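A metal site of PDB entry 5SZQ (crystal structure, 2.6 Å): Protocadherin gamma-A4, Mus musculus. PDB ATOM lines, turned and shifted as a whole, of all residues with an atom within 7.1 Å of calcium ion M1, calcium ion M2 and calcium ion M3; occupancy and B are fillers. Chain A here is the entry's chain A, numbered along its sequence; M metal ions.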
ATOM      1  N   GLU A  16     -31.220  19.564  12.582  1.00  0.00           N
ATOM      2  CA  GLU A  16     -32.482  18.848  12.388  1.00  0.00           C
ATOM      3  C   GLU A  16     -33.505  19.126  13.482  1.00  0.00           C
ATOM      4  O   GLU A  16     -34.700  18.963  13.255  1.00  0.00           O
ATOM      5  CB  GLU A  16     -32.212  17.340  12.303  1.00  0.00           C
ATOM      6  CG  GLU A  16     -31.667  16.754  13.600  1.00  0.00           C
ATOM      7  CD  GLU A  16     -31.635  15.242  13.570  1.00  0.00           C
ATOM      8  OE1 GLU A  16     -32.418  14.650  12.805  1.00  0.00           O
ATOM      9  OE2 GLU A  16     -30.812  14.637  14.301  1.00  0.00           O
ATOM     10  N   ASN A  17     -33.056  19.573  14.657  1.00  0.00           N
ATOM     11  CA  ASN A  17     -33.934  19.764  15.802  1.00  0.00           C
ATOM     12  C   ASN A  17     -34.621  21.123  15.810  1.00  0.00           C
ATOM     13  O   ASN A  17     -35.128  21.537  16.862  1.00  0.00           O
ATOM     14  CB  ASN A  17     -33.156  19.583  17.108  1.00  0.00           C
ATOM     15  CG  ASN A  17     -32.177  20.721  17.362  1.00  0.00           C
ATOM     16  OD1 ASN A  17     -31.668  21.347  16.432  1.00  0.00           O
ATOM     17  ND2 ASN A  17     -31.901  21.005  18.637  1.00  0.00           N
ATOM     18  N   GLU A  69     -41.248  18.835  11.314  1.00  0.00           N
ATOM     19  CA  GLU A  69     -39.921  18.574  11.859  1.00  0.00           C
ATOM     20  C   GLU A  69     -39.042  17.860  10.839  1.00  0.00           C
ATOM     21  O   GLU A  69     -39.462  16.884  10.210  1.00  0.00           O
ATOM     22  CB  GLU A  69     -40.042  17.742  13.142  1.00  0.00           C
ATOM     23  CG  GLU A  69     -38.707  17.325  13.764  1.00  0.00           C
ATOM     24  CD  GLU A  69     -38.067  18.428  14.593  1.00  0.00           C
ATOM     25  OE1 GLU A  69     -38.405  19.615  14.378  1.00  0.00           O
ATOM     26  OE2 GLU A  69     -37.216  18.095  15.456  1.00  0.00           O
ATOM     27  N   LEU A  70     -37.821  18.370  10.684  1.00  0.00           N
ATOM     28  CA  LEU A  70     -36.867  17.801   9.748  1.00  0.00           C
ATOM     29  C   LEU A  70     -36.033  16.754  10.453  1.00  0.00           C
ATOM     30  O   LEU A  70     -35.395  17.033  11.482  1.00  0.00           O
ATOM     31  CB  LEU A  70     -35.963  18.891   9.163  1.00  0.00           C
ATOM     32  CG  LEU A  70     -36.660  20.167   8.660  1.00  0.00           C
ATOM     33  CD1 LEU A  70     -35.652  21.174   8.130  1.00  0.00           C
ATOM     34  CD2 LEU A  70     -37.686  19.838   7.589  1.00  0.00           C
ATOM     35  N   ASP A  71     -36.024  15.540   9.922  1.00  0.00           N
ATOM     36  CA  ASP A  71     -35.247  14.447  10.478  1.00  0.00           C
ATOM     37  C   ASP A  71     -34.048  14.236   9.561  1.00  0.00           C
ATOM     38  O   ASP A  71     -34.225  13.892   8.387  1.00  0.00           O
ATOM     39  CB  ASP A  71     -36.092  13.183  10.592  1.00  0.00           C
ATOM     40  CG  ASP A  71     -35.516  12.192  11.578  1.00  0.00           C
ATOM     41  OD1 ASP A  71     -35.092  12.618  12.672  1.00  0.00           O
ATOM     42  OD2 ASP A  71     -35.483  10.987  11.247  1.00  0.00           O
ATOM     43  N   TYR A  72     -32.839  14.471  10.087  1.00  0.00           N
ATOM     44  CA  TYR A  72     -31.637  14.235   9.294  1.00  0.00           C
ATOM     45  C   TYR A  72     -31.609  12.802   8.787  1.00  0.00           C
ATOM     46  O   TYR A  72     -31.209  12.543   7.643  1.00  0.00           O
ATOM     47  CB  TYR A  72     -30.382  14.535  10.118  1.00  0.00           C
ATOM     48  CG  TYR A  72     -29.062  14.344   9.374  1.00  0.00           C
ATOM     49  CD1 TYR A  72     -28.349  15.436   8.911  1.00  0.00           C
ATOM     50  CD2 TYR A  72     -28.526  13.077   9.160  1.00  0.00           C
ATOM     51  CE1 TYR A  72     -27.147  15.280   8.232  1.00  0.00           C
ATOM     52  CE2 TYR A  72     -27.330  12.906   8.489  1.00  0.00           C
ATOM     53  CZ  TYR A  72     -26.650  14.006   8.027  1.00  0.00           C
ATOM     54  OH  TYR A  72     -25.454  13.844   7.360  1.00  0.00           O
ATOM     55  N   GLU A  73     -32.022  11.861   9.628  1.00  0.00           N
ATOM     56  CA  GLU A  73     -32.052  10.450   9.252  1.00  0.00           C
ATOM     57  C   GLU A  73     -33.045  10.159   8.129  1.00  0.00           C
ATOM     58  O   GLU A  73     -32.975   9.081   7.535  1.00  0.00           O
ATOM     59  CB  GLU A  73     -32.380   9.592  10.478  1.00  0.00           C
ATOM     60  CG  GLU A  73     -31.250   9.503  11.492  1.00  0.00           C
ATOM     61  CD  GLU A  73     -30.997  10.802  12.225  1.00  0.00           C
ATOM     62  OE1 GLU A  73     -31.979  11.399  12.716  1.00  0.00           O
ATOM     63  OE2 GLU A  73     -29.830  11.232  12.303  1.00  0.00           O
ATOM     64  N   ASP A  74     -33.955  11.092   7.843  1.00  0.00           N
ATOM     65  CA  ASP A  74     -34.871  10.931   6.718  1.00  0.00           C
ATOM     66  C   ASP A  74     -34.281  11.519   5.437  1.00  0.00           C
ATOM     67  O   ASP A  74     -34.302  10.867   4.385  1.00  0.00           O
ATOM     68  CB  ASP A  74     -36.212  11.597   7.037  1.00  0.00           C
ATOM     69  CG  ASP A  74     -37.273  11.311   5.985  1.00  0.00           C
ATOM     70  OD1 ASP A  74     -37.304  10.176   5.444  1.00  0.00           O
ATOM     71  OD2 ASP A  74     -38.087  12.223   5.692  1.00  0.00           O
ATOM     72  N   LEU A 101     -28.382  19.559   9.349  1.00  0.00           N
ATOM     73  CA  LEU A 101     -27.250  19.083  10.126  1.00  0.00           C
ATOM     74  C   LEU A 101     -27.700  17.989  11.073  1.00  0.00           C
ATOM     75  O   LEU A 101     -28.867  17.911  11.478  1.00  0.00           O
ATOM     76  CB  LEU A 101     -26.617  20.234  10.921  1.00  0.00           C
ATOM     77  CG  LEU A 101     -26.195  21.457  10.097  1.00  0.00           C
ATOM     78  CD1 LEU A 101     -25.574  22.520  10.983  1.00  0.00           C
ATOM     79  CD2 LEU A 101     -25.253  21.069   8.959  1.00  0.00           C
ATOM     80  N   ASP A 102     -26.765  17.108  11.420  1.00  0.00           N
ATOM     81  CA  ASP A 102     -27.060  15.954  12.267  1.00  0.00           C
ATOM     82  C   ASP A 102     -26.981  16.351  13.735  1.00  0.00           C
ATOM     83  O   ASP A 102     -26.012  16.982  14.170  1.00  0.00           O
ATOM     84  CB  ASP A 102     -26.081  14.825  11.967  1.00  0.00           C
ATOM     85  CG  ASP A 102     -26.221  13.673  12.935  1.00  0.00           C
ATOM     86  OD1 ASP A 102     -25.211  12.971  13.175  1.00  0.00           O
ATOM     87  OD2 ASP A 102     -27.330  13.472  13.473  1.00  0.00           O
ATOM     88  N   VAL A 103     -28.014  15.977  14.491  1.00  0.00           N
ATOM     89  CA  VAL A 103     -28.052  16.153  15.935  1.00  0.00           C
ATOM     90  C   VAL A 103     -28.131  14.775  16.569  1.00  0.00           C
ATOM     91  O   VAL A 103     -28.913  13.927  16.114  1.00  0.00           O
ATOM     92  CB  VAL A 103     -29.240  17.030  16.376  1.00  0.00           C
ATOM     93  CG1 VAL A 103     -29.296  17.125  17.894  1.00  0.00           C
ATOM     94  CG2 VAL A 103     -29.137  18.413  15.760  1.00  0.00           C
ATOM     95  N   ASN A 104     -27.316  14.543  17.590  1.00  0.00           N
ATOM     96  CA  ASN A 104     -27.313  13.252  18.291  1.00  0.00           C
ATOM     97  C   ASN A 104     -28.596  13.147  19.110  1.00  0.00           C
ATOM     98  O   ASN A 104     -28.638  13.414  20.310  1.00  0.00           O
ATOM     99  CB  ASN A 104     -26.071  13.126  19.172  1.00  0.00           C
ATOM    100  CG  ASN A 104     -25.967  11.778  19.850  1.00  0.00           C
ATOM    101  OD1 ASN A 104     -26.574  10.807  19.410  1.00  0.00           O
ATOM    102  ND2 ASN A 104     -25.202  11.710  20.936  1.00  0.00           N
ATOM    103  N   ASP A 105     -29.666  12.728  18.435  1.00  0.00           N
ATOM    104  CA  ASP A 105     -30.971  12.565  19.065  1.00  0.00           C
ATOM    105  C   ASP A 105     -31.474  11.120  19.045  1.00  0.00           C
ATOM    106  O   ASP A 105     -32.646  10.883  19.337  1.00  0.00           O
ATOM    107  CB  ASP A 105     -32.009  13.483  18.404  1.00  0.00           C
ATOM    108  CG  ASP A 105     -32.186  13.184  16.920  1.00  0.00           C
ATOM    109  OD1 ASP A 105     -32.630  14.107  16.203  1.00  0.00           O
ATOM    110  OD2 ASP A 105     -31.890  12.055  16.480  1.00  0.00           O
ATOM    111  N   ASN A 106     -30.611  10.153  18.706  1.00  0.00           N
ATOM    112  CA  ASN A 106     -30.987   8.744  18.728  1.00  0.00           C
ATOM    113  C   ASN A 106     -29.945   7.980  19.535  1.00  0.00           C
ATOM    114  O   ASN A 106     -28.803   7.838  19.099  1.00  0.00           O
ATOM    115  CB  ASN A 106     -31.091   8.169  17.305  1.00  0.00           C
ATOM    116  CG  ASN A 106     -32.385   8.558  16.611  1.00  0.00           C
ATOM    117  OD1 ASN A 106     -33.362   8.952  17.251  1.00  0.00           O
ATOM    118  ND2 ASN A 106     -32.394   8.452  15.293  1.00  0.00           N
ATOM    119  N   ALA A 107     -30.340   7.501  20.719  1.00  0.00           N
ATOM    120  CA  ALA A 107     -29.448   6.668  21.499  1.00  0.00           C
ATOM    121  C   ALA A 107     -29.226   5.327  20.786  1.00  0.00           C
ATOM    122  O   ALA A 107     -30.098   4.876  20.033  1.00  0.00           O
ATOM    123  CB  ALA A 107     -30.013   6.439  22.895  1.00  0.00           C
ATOM    124  N   PRO A 108     -28.072   4.691  20.985  1.00  0.00           N
ATOM    125  CA  PRO A 108     -27.800   3.434  20.292  1.00  0.00           C
ATOM    126  C   PRO A 108     -28.802   2.352  20.650  1.00  0.00           C
ATOM    127  O   PRO A 108     -29.293   2.276  21.781  1.00  0.00           O
ATOM    128  CB  PRO A 108     -26.388   3.066  20.751  1.00  0.00           C
ATOM    129  CG  PRO A 108     -26.157   3.875  21.984  1.00  0.00           C
ATOM    130  CD  PRO A 108     -26.919   5.142  21.772  1.00  0.00           C
ATOM    131  N   ASP A 136     -26.762   2.238  15.423  1.00  0.00           N
ATOM    132  CA  ASP A 136     -27.162   3.604  15.761  1.00  0.00           C
ATOM    133  C   ASP A 136     -27.631   4.307  14.490  1.00  0.00           C
ATOM    134  O   ASP A 136     -26.968   4.215  13.447  1.00  0.00           O
ATOM    135  CB  ASP A 136     -26.012   4.373  16.414  1.00  0.00           C
ATOM    136  CG  ASP A 136     -26.458   5.701  17.013  1.00  0.00           C
ATOM    137  OD1 ASP A 136     -27.676   5.927  17.157  1.00  0.00           O
ATOM    138  OD2 ASP A 136     -25.569   6.520  17.362  1.00  0.00           O
ATOM    139  N   SER A 137     -28.759   5.009  14.584  1.00  0.00           N
ATOM    140  CA  SER A 137     -29.329   5.688  13.438  1.00  0.00           C
ATOM    141  C   SER A 137     -28.616   7.008  13.130  1.00  0.00           C
ATOM    142  O   SER A 137     -28.691   7.485  11.996  1.00  0.00           O
ATOM    143  CB  SER A 137     -30.825   5.945  13.676  1.00  0.00           C
ATOM    144  OG  SER A 137     -31.514   4.720  13.858  1.00  0.00           O
ATOM    145  N   ASP A 138     -27.938   7.591  14.107  1.00  0.00           N
ATOM    146  CA  ASP A 138     -27.268   8.866  13.884  1.00  0.00           C
ATOM    147  C   ASP A 138     -26.032   8.673  13.008  1.00  0.00           C
ATOM    148  O   ASP A 138     -25.580   7.553  12.748  1.00  0.00           O
ATOM    149  CB  ASP A 138     -26.903   9.536  15.206  1.00  0.00           C
ATOM    150  CG  ASP A 138     -28.118   9.983  15.993  1.00  0.00           C
ATOM    151  OD1 ASP A 138     -28.800  10.930  15.535  1.00  0.00           O
ATOM    152  OD2 ASP A 138     -28.382   9.402  17.068  1.00  0.00           O
ATOM    153  N   SER A 139     -25.468   9.790  12.558  1.00  0.00           N
ATOM    154  CA  SER A 139     -24.364   9.796  11.606  1.00  0.00           C
ATOM    155  C   SER A 139     -23.104  10.363  12.238  1.00  0.00           C
ATOM    156  O   SER A 139     -23.147  11.021  13.289  1.00  0.00           O
ATOM    157  CB  SER A 139     -24.733  10.607  10.361  1.00  0.00           C
ATOM    158  OG  SER A 139     -26.072  10.342   9.967  1.00  0.00           O
ATOM    159  N   GLU A 141     -19.617  10.882  14.213  1.00  0.00           N
ATOM    160  CA  GLU A 141     -19.261  10.462  15.565  1.00  0.00           C
ATOM    161  C   GLU A 141     -20.491  10.277  16.446  1.00  0.00           C
ATOM    162  O   GLU A 141     -20.419   9.545  17.436  1.00  0.00           O
ATOM    163  CB  GLU A 141     -18.297  11.461  16.208  1.00  0.00           C
ATOM    164  CG  GLU A 141     -16.852  11.309  15.760  1.00  0.00           C
ATOM    165  CD  GLU A 141     -15.892  12.142  16.593  1.00  0.00           C
ATOM    166  OE1 GLU A 141     -16.350  13.094  17.260  1.00  0.00           O
ATOM    167  OE2 GLU A 141     -14.684  11.824  16.594  1.00  0.00           O
ATOM    168  N   ASN A 142     -21.608  10.928  16.105  1.00  0.00           N
ATOM    169  CA  ASN A 142     -22.859  10.658  16.784  1.00  0.00           C
ATOM    170  C   ASN A 142     -23.357   9.238  16.545  1.00  0.00           C
ATOM    171  O   ASN A 142     -24.260   8.790  17.250  1.00  0.00           O
ATOM    172  CB  ASN A 142     -23.945  11.657  16.345  1.00  0.00           C
ATOM    173  CG  ASN A 142     -23.534  13.112  16.514  1.00  0.00           C
ATOM    174  OD1 ASN A 142     -22.605  13.429  17.258  1.00  0.00           O
ATOM    175  ND2 ASN A 142     -24.239  14.009  15.825  1.00  0.00           N
ATOM    176  N   GLY A 143     -22.785   8.533  15.561  1.00  0.00           N
ATOM    177  CA  GLY A 143     -23.245   7.219  15.174  1.00  0.00           C
ATOM    178  C   GLY A 143     -22.303   6.089  15.558  1.00  0.00           C
ATOM    179  O   GLY A 143     -22.739   4.939  15.679  1.00  0.00           O
ATOM    180  N   LEU A 144     -21.015   6.389  15.722  1.00  0.00           N
ATOM    181  CA  LEU A 144     -20.097   5.398  16.254  1.00  0.00           C
ATOM    182  C   LEU A 144     -20.481   5.048  17.685  1.00  0.00           C
ATOM    183  O   LEU A 144     -21.035   5.876  18.409  1.00  0.00           O
ATOM    184  CB  LEU A 144     -18.656   5.910  16.187  1.00  0.00           C
ATOM    185  CG  LEU A 144     -18.061   6.149  14.798  1.00  0.00           C
ATOM    186  CD1 LEU A 144     -16.591   6.524  14.912  1.00  0.00           C
ATOM    187  CD2 LEU A 144     -18.235   4.928  13.891  1.00  0.00           C
ATOM    188  N   ASP A 189     -22.489   6.344  23.235  1.00  0.00           N
ATOM    189  CA  ASP A 189     -22.353   7.125  22.016  1.00  0.00           C
ATOM    190  C   ASP A 189     -21.131   8.009  22.103  1.00  0.00           C
ATOM    191  O   ASP A 189     -20.737   8.462  23.184  1.00  0.00           O
ATOM    192  CB  ASP A 189     -23.608   7.973  21.794  1.00  0.00           C
ATOM    193  CG  ASP A 189     -23.732   8.481  20.393  1.00  0.00           C
ATOM    194  OD1 ASP A 189     -22.712   8.511  19.684  1.00  0.00           O
ATOM    195  OD2 ASP A 189     -24.856   8.856  20.002  1.00  0.00           O
ATOM    196  N   GLN A 190     -20.521   8.288  20.942  1.00  0.00           N
ATOM    197  CA  GLN A 190     -19.337   9.129  20.875  1.00  0.00           C
ATOM    198  C   GLN A 190     -19.669  10.600  20.622  1.00  0.00           C
ATOM    199  O   GLN A 190     -18.859  11.475  20.954  1.00  0.00           O
ATOM    200  CB  GLN A 190     -18.395   8.587  19.784  1.00  0.00           C
ATOM    201  CG  GLN A 190     -17.227   9.498  19.399  1.00  0.00           C
ATOM    202  CD  GLN A 190     -16.189   9.648  20.502  1.00  0.00           C
ATOM    203  OE1 GLN A 190     -15.922   8.706  21.246  1.00  0.00           O
ATOM    204  NE2 GLN A 190     -15.604  10.842  20.602  1.00  0.00           N
ATOM    205  N   GLY A 191     -20.846  10.897  20.078  1.00  0.00           N
ATOM    206  CA  GLY A 191     -21.199  12.281  19.793  1.00  0.00           C
ATOM    207  C   GLY A 191     -21.653  13.028  21.042  1.00  0.00           C
ATOM    208  O   GLY A 191     -22.354  12.484  21.900  1.00  0.00           O
ATOM    209  N   LEU A 195     -25.001   9.724  24.379  1.00  0.00           N
ATOM    210  CA  LEU A 195     -26.251   9.060  24.716  1.00  0.00           C
ATOM    211  C   LEU A 195     -25.994   7.577  24.909  1.00  0.00           C
ATOM    212  O   LEU A 195     -25.450   6.914  24.020  1.00  0.00           O
ATOM    213  CB  LEU A 195     -27.315   9.262  23.638  1.00  0.00           C
ATOM    214  CG  LEU A 195     -28.008  10.630  23.629  1.00  0.00           C
ATOM    215  CD1 LEU A 195     -29.139  10.636  22.624  1.00  0.00           C
ATOM    216  CD2 LEU A 195     -28.502  10.973  25.022  1.00  0.00           C
HETATM  217 CA    CA M   1     -26.482   8.483  18.619  1.00  0.00          CA
HETATM  218 CA    CA M   2     -30.049  12.472  14.133  1.00  0.00          CA
HETATM  219 CA    CA M   3     -33.415  12.754  14.243  1.00  0.00          CA
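Calcium ion M2 is bound by the side-chain carboxylate (OE2) of Glu 73 (2.2 Å), the side-chain carboxylate (OE2) of Glu 16 (2.3 Å), the side-chain carboxylate (OD1) of Asp 138 (2.4 Å), the side-chain carboxylate (OE1) of Glu 73 (2.6 Å) and the backbone carbonyl oxygen (O) of Val 103 (2.7 Å). Slightly farther from calcium ion M2 lies the side-chain carboxylate (OD2) of Asp 102 (3.0 Å). Slightly farther from calcium ion M2 lies OD2 of Asp 105 (3.0 Å).
N of Asp 189 lies close to O of Leu 195 (3.1 Å). OD1 of Asp 189 sits at hydrogen-bond distance from N of Gly 191 (3.1 Å). The backbone NH (N) of Tyr 72 sits close to the side-chain carboxylate (OE1) of Glu 16. The backbone carbonyl oxygen of Leu 70 sits close to the backbone carbonyl oxygen of Glu 16. The backbone NH (N) of Glu 16 lies within hydrogen-bond range of the backbone carbonyl oxygen (O) of Leu 101. ND2 of Asn 104 lies within hydrogen-bond range of O of Gly 191, 3.1 Å away. The side-chain carboxylate (OD1) of Asp 102 sits at hydrogen-bond distance from the side-chain amide nitrogen (ND2) of Asn 142 (3.0 Å). N of Ser 139 is in hydrogen-bond range of OD1 of Asp 102.
Calcium ion M1 is bound by the side-chain carboxylate (OD2) of Asp 189, the backbone carbonyl oxygen (O) of Asn 106, the side-chain amide oxygen (OD1) of Asn 104, the side-chain carboxylate (OD2) of Asp 136, the side-chain carboxylate (OD2) of Asp 138 and the backbone carbonyl oxygen (O) of Asn 142.
Within 4 Å of calcium ion M1: Asn 104, Asn 106, Asp 136, Asp 138, Asn 142 and Asp 189. Along chain A the residues within 4 Å of calcium ion M1 span positions 104 to 189. The nearest printed residue that does not touch calcium ion M1 is Ala 107 (4.5 Å).
Of the 28 residues printed, 6 come within 4 Å of calcium ion M2. The nearest printed residue that does not touch calcium ion M2 is Tyr 72 (4.5 Å).
Within 4 Å of calcium ion M3: Glu 16, Asp 71, Glu 73 and Asp 105. Along chain A the residues within 4 Å of calcium ion M3 span positions 16 to 105.
Calcium ion M3 is bound by OD1 of Asp 71 (2.3 Å), OE1 of Glu 73 (2.5 Å), OD1 of Asp 105 (2.5 Å), OE1 of Glu 16 (2.6 Å) and OD2 of Asp 105 (2.8 Å).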
